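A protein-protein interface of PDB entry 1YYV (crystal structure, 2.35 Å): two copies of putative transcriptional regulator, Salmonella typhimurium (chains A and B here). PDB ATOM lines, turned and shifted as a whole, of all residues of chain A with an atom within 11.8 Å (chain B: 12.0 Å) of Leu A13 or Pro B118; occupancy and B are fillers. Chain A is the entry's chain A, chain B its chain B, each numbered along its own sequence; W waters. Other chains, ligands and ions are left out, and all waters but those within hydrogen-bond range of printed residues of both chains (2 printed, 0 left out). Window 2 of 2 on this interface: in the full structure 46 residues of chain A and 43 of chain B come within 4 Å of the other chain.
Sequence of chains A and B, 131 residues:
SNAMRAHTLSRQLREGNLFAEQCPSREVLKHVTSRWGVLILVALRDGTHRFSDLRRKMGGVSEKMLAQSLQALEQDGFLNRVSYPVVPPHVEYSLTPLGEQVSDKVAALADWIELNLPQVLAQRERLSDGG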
ATOM      1  N   GLN A  12      33.645 -15.061 -28.068  1.00  0.00           N
ATOM      2  CA  GLN A  12      33.155 -16.468 -27.897  1.00  0.00           C
ATOM      3  C   GLN A  12      31.711 -16.453 -27.384  1.00  0.00           C
ATOM      4  O   GLN A  12      31.491 -16.252 -26.190  1.00  0.00           O
ATOM      5  CB  GLN A  12      34.055 -17.235 -26.906  1.00  0.00           C
ATOM      6  CG  GLN A  12      34.493 -16.376 -25.689  1.00  0.00           C
ATOM      7  CD  GLN A  12      34.637 -17.165 -24.374  1.00  0.00           C
ATOM      8  OE1 GLN A  12      35.770 -17.387 -23.899  1.00  0.00           O
ATOM      9  NE2 GLN A  12      33.487 -17.577 -23.767  1.00  0.00           N
ATOM     10  N   LEU A  13      30.723 -16.679 -28.257  1.00  0.00           N
ATOM     11  CA  LEU A  13      29.321 -16.669 -27.773  1.00  0.00           C
ATOM     12  C   LEU A  13      28.778 -18.035 -27.263  1.00  0.00           C
ATOM     13  O   LEU A  13      27.712 -18.553 -27.642  1.00  0.00           O
ATOM     14  CB  LEU A  13      28.378 -15.882 -28.681  1.00  0.00           C
ATOM     15  CG  LEU A  13      28.766 -14.377 -28.658  1.00  0.00           C
ATOM     16  CD1 LEU A  13      27.652 -13.439 -29.213  1.00  0.00           C
ATOM     17  CD2 LEU A  13      29.262 -13.869 -27.276  1.00  0.00           C
ATOM     18  N   ARG A  14      29.559 -18.586 -26.352  1.00  0.00           N
ATOM     19  CA  ARG A  14      29.233 -19.806 -25.692  1.00  0.00           C
ATOM     20  C   ARG A  14      28.579 -19.493 -24.345  1.00  0.00           C
ATOM     21  O   ARG A  14      28.688 -18.368 -23.810  1.00  0.00           O
ATOM     22  CB  ARG A  14      30.518 -20.591 -25.493  1.00  0.00           C
ATOM     23  CG  ARG A  14      31.225 -20.801 -26.787  1.00  0.00           C
ATOM     24  CD  ARG A  14      32.712 -20.944 -26.552  1.00  0.00           C
ATOM     25  NE  ARG A  14      33.119 -22.349 -26.592  1.00  0.00           N
ATOM     26  CZ  ARG A  14      33.680 -22.939 -27.646  1.00  0.00           C
ATOM     27  NH1 ARG A  14      33.925 -22.253 -28.775  1.00  0.00           N
ATOM     28  NH2 ARG A  14      34.007 -24.220 -27.559  1.00  0.00           N
ATOM     29  N   GLU A  15      27.887 -20.495 -23.825  1.00  0.00           N
ATOM     30  CA  GLU A  15      27.488 -20.487 -22.425  1.00  0.00           C
ATOM     31  C   GLU A  15      28.708 -20.814 -21.593  1.00  0.00           C
ATOM     32  O   GLU A  15      29.611 -21.524 -22.049  1.00  0.00           O
ATOM     33  CB  GLU A  15      26.316 -21.447 -22.181  1.00  0.00           C
ATOM     34  CG  GLU A  15      25.008 -20.889 -22.846  1.00  0.00           C
ATOM     35  CD  GLU A  15      23.751 -21.760 -22.643  1.00  0.00           C
ATOM     36  OE1 GLU A  15      23.598 -22.431 -21.593  1.00  0.00           O
ATOM     37  OE2 GLU A  15      22.896 -21.757 -23.557  1.00  0.00           O
ATOM     38  N   GLY A  16      28.784 -20.236 -20.402  1.00  0.00           N
ATOM     39  CA  GLY A  16      29.958 -20.408 -19.594  1.00  0.00           C
ATOM     40  C   GLY A  16      30.073 -21.753 -18.916  1.00  0.00           C
ATOM     41  O   GLY A  16      29.080 -22.521 -18.734  1.00  0.00           O
ATOM     42  N   ASN A  17      31.306 -22.021 -18.508  1.00  0.00           N
ATOM     43  CA  ASN A  17      31.581 -23.118 -17.633  1.00  0.00           C
ATOM     44  C   ASN A  17      32.512 -22.672 -16.470  1.00  0.00           C
ATOM     45  O   ASN A  17      33.716 -22.572 -16.642  1.00  0.00           O
ATOM     46  CB  ASN A  17      32.151 -24.259 -18.454  1.00  0.00           C
ATOM     47  CG  ASN A  17      32.491 -25.472 -17.613  1.00  0.00           C
ATOM     48  OD1 ASN A  17      32.148 -25.558 -16.442  1.00  0.00           O
ATOM     49  ND2 ASN A  17      33.181 -26.394 -18.205  1.00  0.00           N
ATOM     50  N   LEU A  18      31.934 -22.396 -15.295  1.00  0.00           N
ATOM     51  CA  LEU A  18      32.709 -21.987 -14.126  1.00  0.00           C
ATOM     52  C   LEU A  18      33.817 -22.964 -13.694  1.00  0.00           C
ATOM     53  O   LEU A  18      34.787 -22.540 -13.054  1.00  0.00           O
ATOM     54  CB  LEU A  18      31.773 -21.686 -12.962  1.00  0.00           C
ATOM     55  CG  LEU A  18      31.003 -20.397 -13.206  1.00  0.00           C
ATOM     56  CD1 LEU A  18      29.683 -20.390 -12.364  1.00  0.00           C
ATOM     57  CD2 LEU A  18      31.860 -19.166 -12.906  1.00  0.00           C
ATOM     58  N   CYS A  23      37.442 -19.439 -18.062  1.00  0.00           N
ATOM     59  CA  CYS A  23      36.175 -19.033 -18.644  1.00  0.00           C
ATOM     60  C   CYS A  23      35.841 -17.639 -18.086  1.00  0.00           C
ATOM     61  O   CYS A  23      35.945 -17.417 -16.895  1.00  0.00           O
ATOM     62  CB  CYS A  23      35.047 -20.049 -18.344  1.00  0.00           C
ATOM     63  SG  CYS A  23      33.401 -19.485 -18.955  1.00  0.00           S
ATOM     64  N   PRO A  24      35.420 -16.695 -18.935  1.00  0.00           N
ATOM     65  CA  PRO A  24      35.071 -15.356 -18.395  1.00  0.00           C
ATOM     66  C   PRO A  24      33.876 -15.308 -17.403  1.00  0.00           C
ATOM     67  O   PRO A  24      33.621 -14.262 -16.781  1.00  0.00           O
ATOM     68  CB  PRO A  24      34.757 -14.532 -19.663  1.00  0.00           C
ATOM     69  CG  PRO A  24      35.361 -15.312 -20.819  1.00  0.00           C
ATOM     70  CD  PRO A  24      35.240 -16.768 -20.400  1.00  0.00           C
ATOM     71  N   SER A  25      33.135 -16.399 -17.253  1.00  0.00           N
ATOM     72  CA  SER A  25      32.050 -16.419 -16.263  1.00  0.00           C
ATOM     73  C   SER A  25      32.599 -16.264 -14.844  1.00  0.00           C
ATOM     74  O   SER A  25      31.894 -15.780 -13.940  1.00  0.00           O
ATOM     75  CB  SER A  25      31.218 -17.714 -16.377  1.00  0.00           C
ATOM     76  OG  SER A  25      32.061 -18.856 -16.290  1.00  0.00           O
ATOM     77  N   ARG A  26      33.848 -16.704 -14.647  1.00  0.00           N
ATOM     78  CA  ARG A  26      34.549 -16.552 -13.353  1.00  0.00           C
ATOM     79  C   ARG A  26      34.757 -15.069 -12.979  1.00  0.00           C
ATOM     80  O   ARG A  26      34.637 -14.689 -11.832  1.00  0.00           O
ATOM     81  CB  ARG A  26      35.869 -17.268 -13.405  1.00  0.00           C
ATOM     82  CG  ARG A  26      35.723 -18.759 -13.276  1.00  0.00           C
ATOM     83  CD  ARG A  26      37.080 -19.450 -13.345  1.00  0.00           C
ATOM     84  NE  ARG A  26      36.904 -20.886 -13.121  1.00  0.00           N
ATOM     85  CZ  ARG A  26      37.890 -21.728 -12.837  1.00  0.00           C
ATOM     86  NH1 ARG A  26      39.137 -21.286 -12.739  1.00  0.00           N
ATOM     87  NH2 ARG A  26      37.630 -23.016 -12.665  1.00  0.00           N
ATOM     88  N   VAL A  28      32.783 -12.442 -14.271  1.00  0.00           N
ATOM     89  CA  VAL A  28      31.413 -12.019 -13.955  1.00  0.00           C
ATOM     90  C   VAL A  28      31.015 -12.449 -12.554  1.00  0.00           C
ATOM     91  O   VAL A  28      30.473 -11.672 -11.809  1.00  0.00           O
ATOM     92  CB  VAL A  28      30.409 -12.570 -14.972  1.00  0.00           C
ATOM     93  CG1 VAL A  28      28.947 -12.137 -14.617  1.00  0.00           C
ATOM     94  CG2 VAL A  28      30.869 -12.211 -16.422  1.00  0.00           C
ATOM     95  N   LEU A  29      31.313 -13.675 -12.180  1.00  0.00           N
ATOM     96  CA  LEU A  29      30.999 -14.146 -10.826  1.00  0.00           C
ATOM     97  C   LEU A  29      31.703 -13.318  -9.736  1.00  0.00           C
ATOM     98  O   LEU A  29      31.079 -12.924  -8.791  1.00  0.00           O
ATOM     99  CB  LEU A  29      31.288 -15.640 -10.699  1.00  0.00           C
ATOM    100  CG  LEU A  29      31.313 -16.166  -9.276  1.00  0.00           C
ATOM    101  CD1 LEU A  29      29.897 -16.424  -8.792  1.00  0.00           C
ATOM    102  CD2 LEU A  29      32.213 -17.402  -9.158  1.00  0.00           C
ATOM    103  N   GLN A  75      30.311  -2.275 -17.502  1.00  0.00           N
ATOM    104  CA  GLN A  75      30.806  -2.889 -18.730  1.00  0.00           C
ATOM    105  C   GLN A  75      30.340  -4.322 -18.917  1.00  0.00           C
ATOM    106  O   GLN A  75      30.343  -4.805 -20.054  1.00  0.00           O
ATOM    107  CB  GLN A  75      32.314  -2.675 -19.008  1.00  0.00           C
ATOM    108  CG  GLN A  75      33.263  -3.033 -17.892  1.00  0.00           C
ATOM    109  CD  GLN A  75      34.563  -2.201 -17.923  1.00  0.00           C
ATOM    110  OE1 GLN A  75      34.574  -1.052 -18.378  1.00  0.00           O
ATOM    111  NE2 GLN A  75      35.650  -2.776 -17.388  1.00  0.00           N
ATOM    112  N   ASP A  76      29.895  -4.967 -17.826  1.00  0.00           N
ATOM    113  CA  ASP A  76      29.223  -6.264 -17.898  1.00  0.00           C
ATOM    114  C   ASP A  76      27.796  -6.112 -18.438  1.00  0.00           C
ATOM    115  O   ASP A  76      27.250  -7.032 -19.000  1.00  0.00           O
ATOM    116  CB  ASP A  76      29.214  -6.954 -16.528  1.00  0.00           C
ATOM    117  CG  ASP A  76      30.582  -7.595 -16.168  1.00  0.00           C
ATOM    118  OD1 ASP A  76      31.480  -7.639 -17.039  1.00  0.00           O
ATOM    119  OD2 ASP A  76      30.771  -8.045 -15.003  1.00  0.00           O
ATOM    120  N   GLY A  77      27.199  -4.934 -18.290  1.00  0.00           N
ATOM    121  CA  GLY A  77      25.885  -4.683 -18.874  1.00  0.00           C
ATOM    122  C   GLY A  77      24.770  -4.651 -17.846  1.00  0.00           C
ATOM    123  O   GLY A  77      23.578  -4.767 -18.210  1.00  0.00           O
ATOM    124  N   PHE A  78      25.147  -4.484 -16.572  1.00  0.00           N
ATOM    125  CA  PHE A  78      24.194  -4.571 -15.487  1.00  0.00           C
ATOM    126  C   PHE A  78      23.702  -3.191 -15.037  1.00  0.00           C
ATOM    127  O   PHE A  78      22.675  -3.093 -14.342  1.00  0.00           O
ATOM    128  CB  PHE A  78      24.787  -5.332 -14.285  1.00  0.00           C
ATOM    129  CG  PHE A  78      25.284  -6.731 -14.611  1.00  0.00           C
ATOM    130  CD1 PHE A  78      24.528  -7.605 -15.415  1.00  0.00           C
ATOM    131  CD2 PHE A  78      26.486  -7.183 -14.092  1.00  0.00           C
ATOM    132  CE1 PHE A  78      24.969  -8.885 -15.692  1.00  0.00           C
ATOM    133  CE2 PHE A  78      26.936  -8.467 -14.356  1.00  0.00           C
ATOM    134  CZ  PHE A  78      26.187  -9.318 -15.163  1.00  0.00           C
ATOM    135  N   LEU A  98      18.987  -6.760 -17.844  1.00  0.00           N
ATOM    136  CA  LEU A  98      19.975  -7.807 -17.534  1.00  0.00           C
ATOM    137  C   LEU A  98      20.471  -7.724 -16.079  1.00  0.00           C
ATOM    138  O   LEU A  98      20.660  -8.748 -15.389  1.00  0.00           O
ATOM    139  CB  LEU A  98      21.156  -7.756 -18.529  1.00  0.00           C
ATOM    140  CG  LEU A  98      22.071  -8.991 -18.549  1.00  0.00           C
ATOM    141  CD1 LEU A  98      21.337 -10.216 -19.153  1.00  0.00           C
ATOM    142  CD2 LEU A  98      23.387  -8.717 -19.285  1.00  0.00           C
ATOM    143  N   GLN A 101      17.984  -9.123 -13.469  1.00  0.00           N
ATOM    144  CA  GLN A 101      18.021 -10.586 -13.370  1.00  0.00           C
ATOM    145  C   GLN A 101      19.089 -11.090 -12.406  1.00  0.00           C
ATOM    146  O   GLN A 101      18.783 -11.802 -11.450  1.00  0.00           O
ATOM    147  CB  GLN A 101      18.194 -11.211 -14.755  1.00  0.00           C
ATOM    148  CG  GLN A 101      17.014 -10.926 -15.739  1.00  0.00           C
ATOM    149  CD  GLN A 101      17.257 -11.537 -17.124  1.00  0.00           C
ATOM    150  OE1 GLN A 101      17.810 -12.648 -17.259  1.00  0.00           O
ATOM    151  NE2 GLN A 101      16.853 -10.808 -18.166  1.00  0.00           N
ATOM    152  N   LEU B 109      22.570 -18.969  -9.124  1.00  0.00           N
ATOM    153  CA  LEU B 109      23.397 -17.830  -9.515  1.00  0.00           C
ATOM    154  C   LEU B 109      24.494 -18.255 -10.516  1.00  0.00           C
ATOM    155  O   LEU B 109      24.711 -17.585 -11.540  1.00  0.00           O
ATOM    156  CB  LEU B 109      23.992 -17.114  -8.268  1.00  0.00           C
ATOM    157  CG  LEU B 109      25.047 -16.012  -8.570  1.00  0.00           C
ATOM    158  CD1 LEU B 109      24.470 -14.815  -9.364  1.00  0.00           C
ATOM    159  CD2 LEU B 109      25.672 -15.462  -7.300  1.00  0.00           C
ATOM    160  N   ALA B 110      25.162 -19.379 -10.219  1.00  0.00           N
ATOM    161  CA  ALA B 110      26.163 -19.960 -11.102  1.00  0.00           C
ATOM    162  C   ALA B 110      25.534 -20.234 -12.470  1.00  0.00           C
ATOM    163  O   ALA B 110      26.096 -19.844 -13.493  1.00  0.00           O
ATOM    164  CB  ALA B 110      26.734 -21.268 -10.496  1.00  0.00           C
ATOM    165  N   ASP B 111      24.381 -20.916 -12.486  1.00  0.00           N
ATOM    166  CA  ASP B 111      23.715 -21.214 -13.751  1.00  0.00           C
ATOM    167  C   ASP B 111      23.262 -19.961 -14.516  1.00  0.00           C
ATOM    168  O   ASP B 111      23.411 -19.890 -15.699  1.00  0.00           O
ATOM    169  CB  ASP B 111      22.525 -22.175 -13.559  1.00  0.00           C
ATOM    170  CG  ASP B 111      21.958 -22.669 -14.892  1.00  0.00           C
ATOM    171  OD1 ASP B 111      22.630 -23.512 -15.555  1.00  0.00           O
ATOM    172  OD2 ASP B 111      20.873 -22.200 -15.301  1.00  0.00           O
ATOM    173  N   TRP B 112      22.722 -18.956 -13.841  1.00  0.00           N
ATOM    174  CA  TRP B 112      22.334 -17.710 -14.553  1.00  0.00           C
ATOM    175  C   TRP B 112      23.539 -17.060 -15.238  1.00  0.00           C
ATOM    176  O   TRP B 112      23.463 -16.628 -16.400  1.00  0.00           O
ATOM    177  CB  TRP B 112      21.691 -16.715 -13.597  1.00  0.00           C
ATOM    178  CG  TRP B 112      21.155 -15.544 -14.305  1.00  0.00           C
ATOM    179  CD1 TRP B 112      19.856 -15.366 -14.731  1.00  0.00           C
ATOM    180  CD2 TRP B 112      21.884 -14.356 -14.708  1.00  0.00           C
ATOM    181  NE1 TRP B 112      19.745 -14.155 -15.372  1.00  0.00           N
ATOM    182  CE2 TRP B 112      20.956 -13.510 -15.371  1.00  0.00           C
ATOM    183  CE3 TRP B 112      23.223 -13.936 -14.580  1.00  0.00           C
ATOM    184  CZ2 TRP B 112      21.322 -12.259 -15.909  1.00  0.00           C
ATOM    185  CZ3 TRP B 112      23.595 -12.690 -15.120  1.00  0.00           C
ATOM    186  CH2 TRP B 112      22.646 -11.879 -15.788  1.00  0.00           C
ATOM    187  N   ILE B 113      24.641 -16.966 -14.500  1.00  0.00           N
ATOM    188  CA  ILE B 113      25.868 -16.385 -15.038  1.00  0.00           C
ATOM    189  C   ILE B 113      26.361 -17.145 -16.253  1.00  0.00           C
ATOM    190  O   ILE B 113      26.650 -16.538 -17.251  1.00  0.00           O
ATOM    191  CB  ILE B 113      27.006 -16.276 -13.957  1.00  0.00           C
ATOM    192  CG1 ILE B 113      26.683 -15.123 -12.968  1.00  0.00           C
ATOM    193  CG2 ILE B 113      28.375 -16.053 -14.643  1.00  0.00           C
ATOM    194  CD1 ILE B 113      27.346 -15.243 -11.665  1.00  0.00           C
ATOM    195  N   GLU B 114      26.441 -18.477 -16.185  1.00  0.00           N
ATOM    196  CA  GLU B 114      26.898 -19.234 -17.319  1.00  0.00           C
ATOM    197  C   GLU B 114      25.941 -19.103 -18.518  1.00  0.00           C
ATOM    198  O   GLU B 114      26.385 -18.917 -19.648  1.00  0.00           O
ATOM    199  CB  GLU B 114      27.059 -20.706 -16.948  1.00  0.00           C
ATOM    200  CG  GLU B 114      28.166 -21.037 -15.970  1.00  0.00           C
ATOM    201  CD  GLU B 114      28.089 -22.547 -15.577  1.00  0.00           C
ATOM    202  OE1 GLU B 114      26.996 -23.109 -15.677  1.00  0.00           O
ATOM    203  OE2 GLU B 114      29.093 -23.198 -15.178  1.00  0.00           O
ATOM    204  N   LEU B 115      24.639 -19.197 -18.252  1.00  0.00           N
ATOM    205  CA  LEU B 115      23.609 -19.064 -19.278  1.00  0.00           C
ATOM    206  C   LEU B 115      23.636 -17.695 -19.976  1.00  0.00           C
ATOM    207  O   LEU B 115      23.525 -17.601 -21.216  1.00  0.00           O
ATOM    208  CB  LEU B 115      22.208 -19.384 -18.688  1.00  0.00           C
ATOM    209  CG  LEU B 115      20.932 -19.157 -19.561  1.00  0.00           C
ATOM    210  CD1 LEU B 115      20.991 -19.889 -20.888  1.00  0.00           C
ATOM    211  CD2 LEU B 115      19.660 -19.572 -18.784  1.00  0.00           C
ATOM    212  N   ASN B 116      23.798 -16.636 -19.182  1.00  0.00           N
ATOM    213  CA  ASN B 116      23.772 -15.311 -19.746  1.00  0.00           C
ATOM    214  C   ASN B 116      25.127 -14.739 -20.114  1.00  0.00           C
ATOM    215  O   ASN B 116      25.231 -13.553 -20.430  1.00  0.00           O
ATOM    216  CB  ASN B 116      23.008 -14.348 -18.843  1.00  0.00           C
ATOM    217  CG  ASN B 116      21.526 -14.607 -18.868  1.00  0.00           C
ATOM    218  OD1 ASN B 116      20.806 -14.020 -19.674  1.00  0.00           O
ATOM    219  ND2 ASN B 116      21.056 -15.520 -17.992  1.00  0.00           N
ATOM    220  N   LEU B 117      26.156 -15.576 -20.091  1.00  0.00           N
ATOM    221  CA  LEU B 117      27.495 -15.102 -20.474  1.00  0.00           C
ATOM    222  C   LEU B 117      27.511 -14.397 -21.878  1.00  0.00           C
ATOM    223  O   LEU B 117      28.075 -13.327 -22.016  1.00  0.00           O
ATOM    224  CB  LEU B 117      28.537 -16.253 -20.383  1.00  0.00           C
ATOM    225  CG  LEU B 117      30.018 -15.865 -20.609  1.00  0.00           C
ATOM    226  CD1 LEU B 117      30.571 -14.742 -19.614  1.00  0.00           C
ATOM    227  CD2 LEU B 117      30.885 -17.110 -20.569  1.00  0.00           C
ATOM    228  N   PRO B 118      26.890 -14.997 -22.925  1.00  0.00           N
ATOM    229  CA  PRO B 118      26.920 -14.279 -24.233  1.00  0.00           C
ATOM    230  C   PRO B 118      26.450 -12.805 -24.224  1.00  0.00           C
ATOM    231  O   PRO B 118      27.049 -11.967 -24.901  1.00  0.00           O
ATOM    232  CB  PRO B 118      26.005 -15.110 -25.138  1.00  0.00           C
ATOM    233  CG  PRO B 118      25.870 -16.447 -24.454  1.00  0.00           C
ATOM    234  CD  PRO B 118      26.192 -16.290 -22.997  1.00  0.00           C
ATOM    235  N   GLN B 119      25.391 -12.496 -23.487  1.00  0.00           N
ATOM    236  CA  GLN B 119      24.900 -11.130 -23.409  1.00  0.00           C
ATOM    237  C   GLN B 119      25.895 -10.222 -22.684  1.00  0.00           C
ATOM    238  O   GLN B 119      26.139  -9.087 -23.119  1.00  0.00           O
ATOM    239  CB  GLN B 119      23.518 -11.079 -22.760  1.00  0.00           C
ATOM    240  CG  GLN B 119      22.440 -11.813 -23.572  1.00  0.00           C
ATOM    241  CD  GLN B 119      22.143 -13.246 -23.046  1.00  0.00           C
ATOM    242  OE1 GLN B 119      22.707 -14.245 -23.524  1.00  0.00           O
ATOM    243  NE2 GLN B 119      21.251 -13.330 -22.055  1.00  0.00           N
ATOM    244  N   VAL B 120      26.501 -10.730 -21.614  1.00  0.00           N
ATOM    245  CA  VAL B 120      27.576 -10.009 -20.914  1.00  0.00           C
ATOM    246  C   VAL B 120      28.770  -9.699 -21.815  1.00  0.00           C
ATOM    247  O   VAL B 120      29.260  -8.588 -21.851  1.00  0.00           O
ATOM    248  CB  VAL B 120      28.020 -10.744 -19.626  1.00  0.00           C
ATOM    249  CG1 VAL B 120      29.295 -10.131 -19.075  1.00  0.00           C
ATOM    250  CG2 VAL B 120      26.908 -10.685 -18.591  1.00  0.00           C
ATOM    251  N   LEU B 121      29.237 -10.677 -22.562  1.00  0.00           N
ATOM    252  CA  LEU B 121      30.357 -10.422 -23.468  1.00  0.00           C
ATOM    253  C   LEU B 121      29.998  -9.408 -24.551  1.00  0.00           C
ATOM    254  O   LEU B 121      30.806  -8.528 -24.846  1.00  0.00           O
ATOM    255  CB  LEU B 121      30.949 -11.719 -24.035  1.00  0.00           C
ATOM    256  CG  LEU B 121      31.577 -12.641 -22.978  1.00  0.00           C
ATOM    257  CD1 LEU B 121      32.042 -13.922 -23.609  1.00  0.00           C
ATOM    258  CD2 LEU B 121      32.721 -11.978 -22.198  1.00  0.00           C
ATOM    259  N   ALA B 122      28.788  -9.501 -25.105  1.00  0.00           N
ATOM    260  CA  ALA B 122      28.294  -8.513 -26.078  1.00  0.00           C
ATOM    261  C   ALA B 122      28.273  -7.076 -25.534  1.00  0.00           C
ATOM    262  O   ALA B 122      28.533  -6.143 -26.274  1.00  0.00           O
ATOM    263  CB  ALA B 122      26.918  -8.904 -26.606  1.00  0.00           C
ATOM    264  N   GLN B 123      27.965  -6.887 -24.255  1.00  0.00           N
ATOM    265  CA  GLN B 123      27.996  -5.547 -23.652  1.00  0.00           C
ATOM    266  C   GLN B 123      29.425  -5.065 -23.400  1.00  0.00           C
ATOM    267  O   GLN B 123      29.705  -3.845 -23.370  1.00  0.00           O
ATOM    268  CB  GLN B 123      27.185  -5.509 -22.350  1.00  0.00           C
ATOM    269  CG  GLN B 123      25.691  -5.470 -22.578  1.00  0.00           C
ATOM    270  CD  GLN B 123      25.309  -4.334 -23.515  1.00  0.00           C
ATOM    271  OE1 GLN B 123      25.545  -3.152 -23.212  1.00  0.00           O
ATOM    272  NE2 GLN B 123      24.741  -4.683 -24.664  1.00  0.00           N
ATOM    273  N   ARG B 124      30.332  -6.025 -23.226  1.00  0.00           N
ATOM    274  CA  ARG B 124      31.743  -5.703 -23.032  1.00  0.00           C
ATOM    275  C   ARG B 124      32.389  -5.037 -24.246  1.00  0.00           C
ATOM    276  O   ARG B 124      33.117  -4.067 -24.084  1.00  0.00           O
ATOM    277  CB  ARG B 124      32.545  -6.909 -22.537  1.00  0.00           C
ATOM    278  CG  ARG B 124      32.256  -7.246 -21.085  1.00  0.00           C
ATOM    279  CD  ARG B 124      33.495  -7.740 -20.366  1.00  0.00           C
ATOM    280  NE  ARG B 124      33.158  -8.637 -19.262  1.00  0.00           N
ATOM    281  CZ  ARG B 124      34.013  -9.034 -18.314  1.00  0.00           C
ATOM    282  NH1 ARG B 124      35.281  -8.582 -18.311  1.00  0.00           N
ATOM    283  NH2 ARG B 124      33.598  -9.848 -17.345  1.00  0.00           N
ATOM    284  N   GLU B 125      32.114  -5.542 -25.447  1.00  0.00           N
ATOM    285  CA  GLU B 125      32.738  -5.002 -26.662  1.00  0.00           C
ATOM    286  C   GLU B 125      32.320  -3.565 -27.014  1.00  0.00           C
ATOM    287  O   GLU B 125      33.169  -2.763 -27.423  1.00  0.00           O
ATOM    288  CB  GLU B 125      32.575  -5.942 -27.865  1.00  0.00           C
ATOM    289  CG  GLU B 125      31.234  -6.619 -27.986  1.00  0.00           C
ATOM    290  CD  GLU B 125      31.294  -7.857 -28.874  1.00  0.00           C
ATOM    291  OE1 GLU B 125      32.383  -8.485 -28.941  1.00  0.00           O
ATOM    292  OE2 GLU B 125      30.253  -8.202 -29.501  1.00  0.00           O
ATOM    293  N   ARG B 126      31.033  -3.253 -26.836  1.00  0.00           N
ATOM    294  CA  ARG B 126      30.496  -1.884 -26.980  1.00  0.00           C
ATOM    295  C   ARG B 126      31.191  -0.835 -26.096  1.00  0.00           C
ATOM    296  O   ARG B 126      31.138  -0.888 -24.857  1.00  0.00           O
ATOM    297  CB  ARG B 126      28.996  -1.883 -26.685  1.00  0.00           C
ATOM    298  CG  ARG B 126      28.271  -3.018 -27.346  1.00  0.00           C
ATOM    299  CD  ARG B 126      27.403  -2.537 -28.473  1.00  0.00           C
ATOM    300  NE  ARG B 126      25.993  -2.723 -28.137  1.00  0.00           N
ATOM    301  CZ  ARG B 126      25.320  -3.863 -28.304  1.00  0.00           C
ATOM    302  NH1 ARG B 126      25.925  -4.942 -28.807  1.00  0.00           N
ATOM    303  NH2 ARG B 126      24.036  -3.929 -27.962  1.00  0.00           N
HETATM  304  O   HOH W   1      29.678 -25.673 -15.501  1.00  0.00           O
HETATM  305  O   HOH W   2      33.922  -5.965 -17.731  1.00  0.00           O
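The side-chain amide oxygen of Gln A101 is in hydrogen-bond range of the indole nitrogen of Trp B112. O of Glu B114 lies within hydrogen-bond range of N of Gly A16 (2.8 Å). The side-chain carboxylate (OD1) of Asp A76 is in salt-bridge range of the guanidinium group (NE) of Arg B124 (3.0 Å). The backbone carbonyl oxygen of Gln A75 lies close to the backbone NH of Arg B124. The backbone NH (N) of Leu A18 lies within hydrogen-bond range of the side-chain carboxylate (OE2) of Glu B114, at 3.0 Å.
The side-chain amide nitrogen (NE2) of Gln B123 lies close to the guanidinium group (NH2) of Arg B126 (3.5 Å). The side-chain amide oxygen of Asn B116 is in hydrogen-bond range of the side-chain amide nitrogen of Gln B119 (2.5 Å).
Leu A13 touches Pro B118. Pro B118 touches Arg A14 (CD to O, 3.3 Å). CD1 of Leu B115 touches OE1 of Glu A15, 3.7 Å away. Cys A23 touches Leu B117. Val B120 touches Val A28. Leu A29 touches Ile B113. Val B120 touches Asp A76 (CA to O, 3.6 Å). Gln B123 touches Gly A77.
Of chain B, only Glu B114 (3.4 Å) and Leu B115 (3.7 Å) come within 4 Å of Glu A15. Printed residues of chain B within 4 Å of Leu A18: Ala B110 and Glu B114. Printed residues of chain B within 4 Å of Leu A29: Ile B113. Of the printed residues of chain A, Ile B113 touches Ser A25 (3.6 Å), Val A28 (3.96 Å) and Leu A29 (3.9 Å). Asn B116 touches just one residue of chain A: Leu A98. Val B120 touches just these residues of chain A: Val A28 (3.7 Å), Asp A76 (3.6 Å) and Phe A78 (3.8 Å). Leu B121 touches just one residue of chain A: Gln A12. Ala B122 touches none of the printed residues of chain A. The nearest residue of chain B that does not touch Leu A13 is Leu B121 (4.2 Å). The nearest residue of chain A that does not touch Pro B118 is Glu A15 (4.4 Å). The nearest printed residue of chain A that does not touch Glu B114 is Ser A25 (4.5 Å).
Of the 18 printed residues of chain B, 12 touch a printed residue of chain A. Along chain B the printed residues that touch a printed residue of chain A span positions 110 to 124. Printed residues of chain A that touch a printed residue of chain B: Gln A12, Leu A13, Arg A14, Glu A15, Gly A16, Asn A17, Leu A18, Cys A23, Ser A25, Val A28, Leu A29, Gln A75, Asp A76, Gly A77, Phe A78, Leu A98 and Gln A101. Hydrophobic or aromatic side chains of chain A within 4 Å of the printed part of chain B: Leu A13, Leu A18, Val A28, Phe A78 and Leu A98. Among the printed residues, Asp or Glu carboxylates within 4 Å of a Lys or Arg side-chain nitrogen of the other chain: Asp A76 with Arg B124.
No position is printed for both chains. Of the 28 pairs that touch across the chains among the printed residues, none has its exchanged pair printed and touching as well.
Water W1 lies within hydrogen-bond range of the side-chain carboxylate of Glu B114 (2.6 Å) and the side-chain amide oxygen of Asn A17 (2.6 Å). Water W2 lies within hydrogen-bond range of the guanidinium group of Arg B124 (3.0 Å) and the side-chain carboxylate of Asp A76 (3.0 Å).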
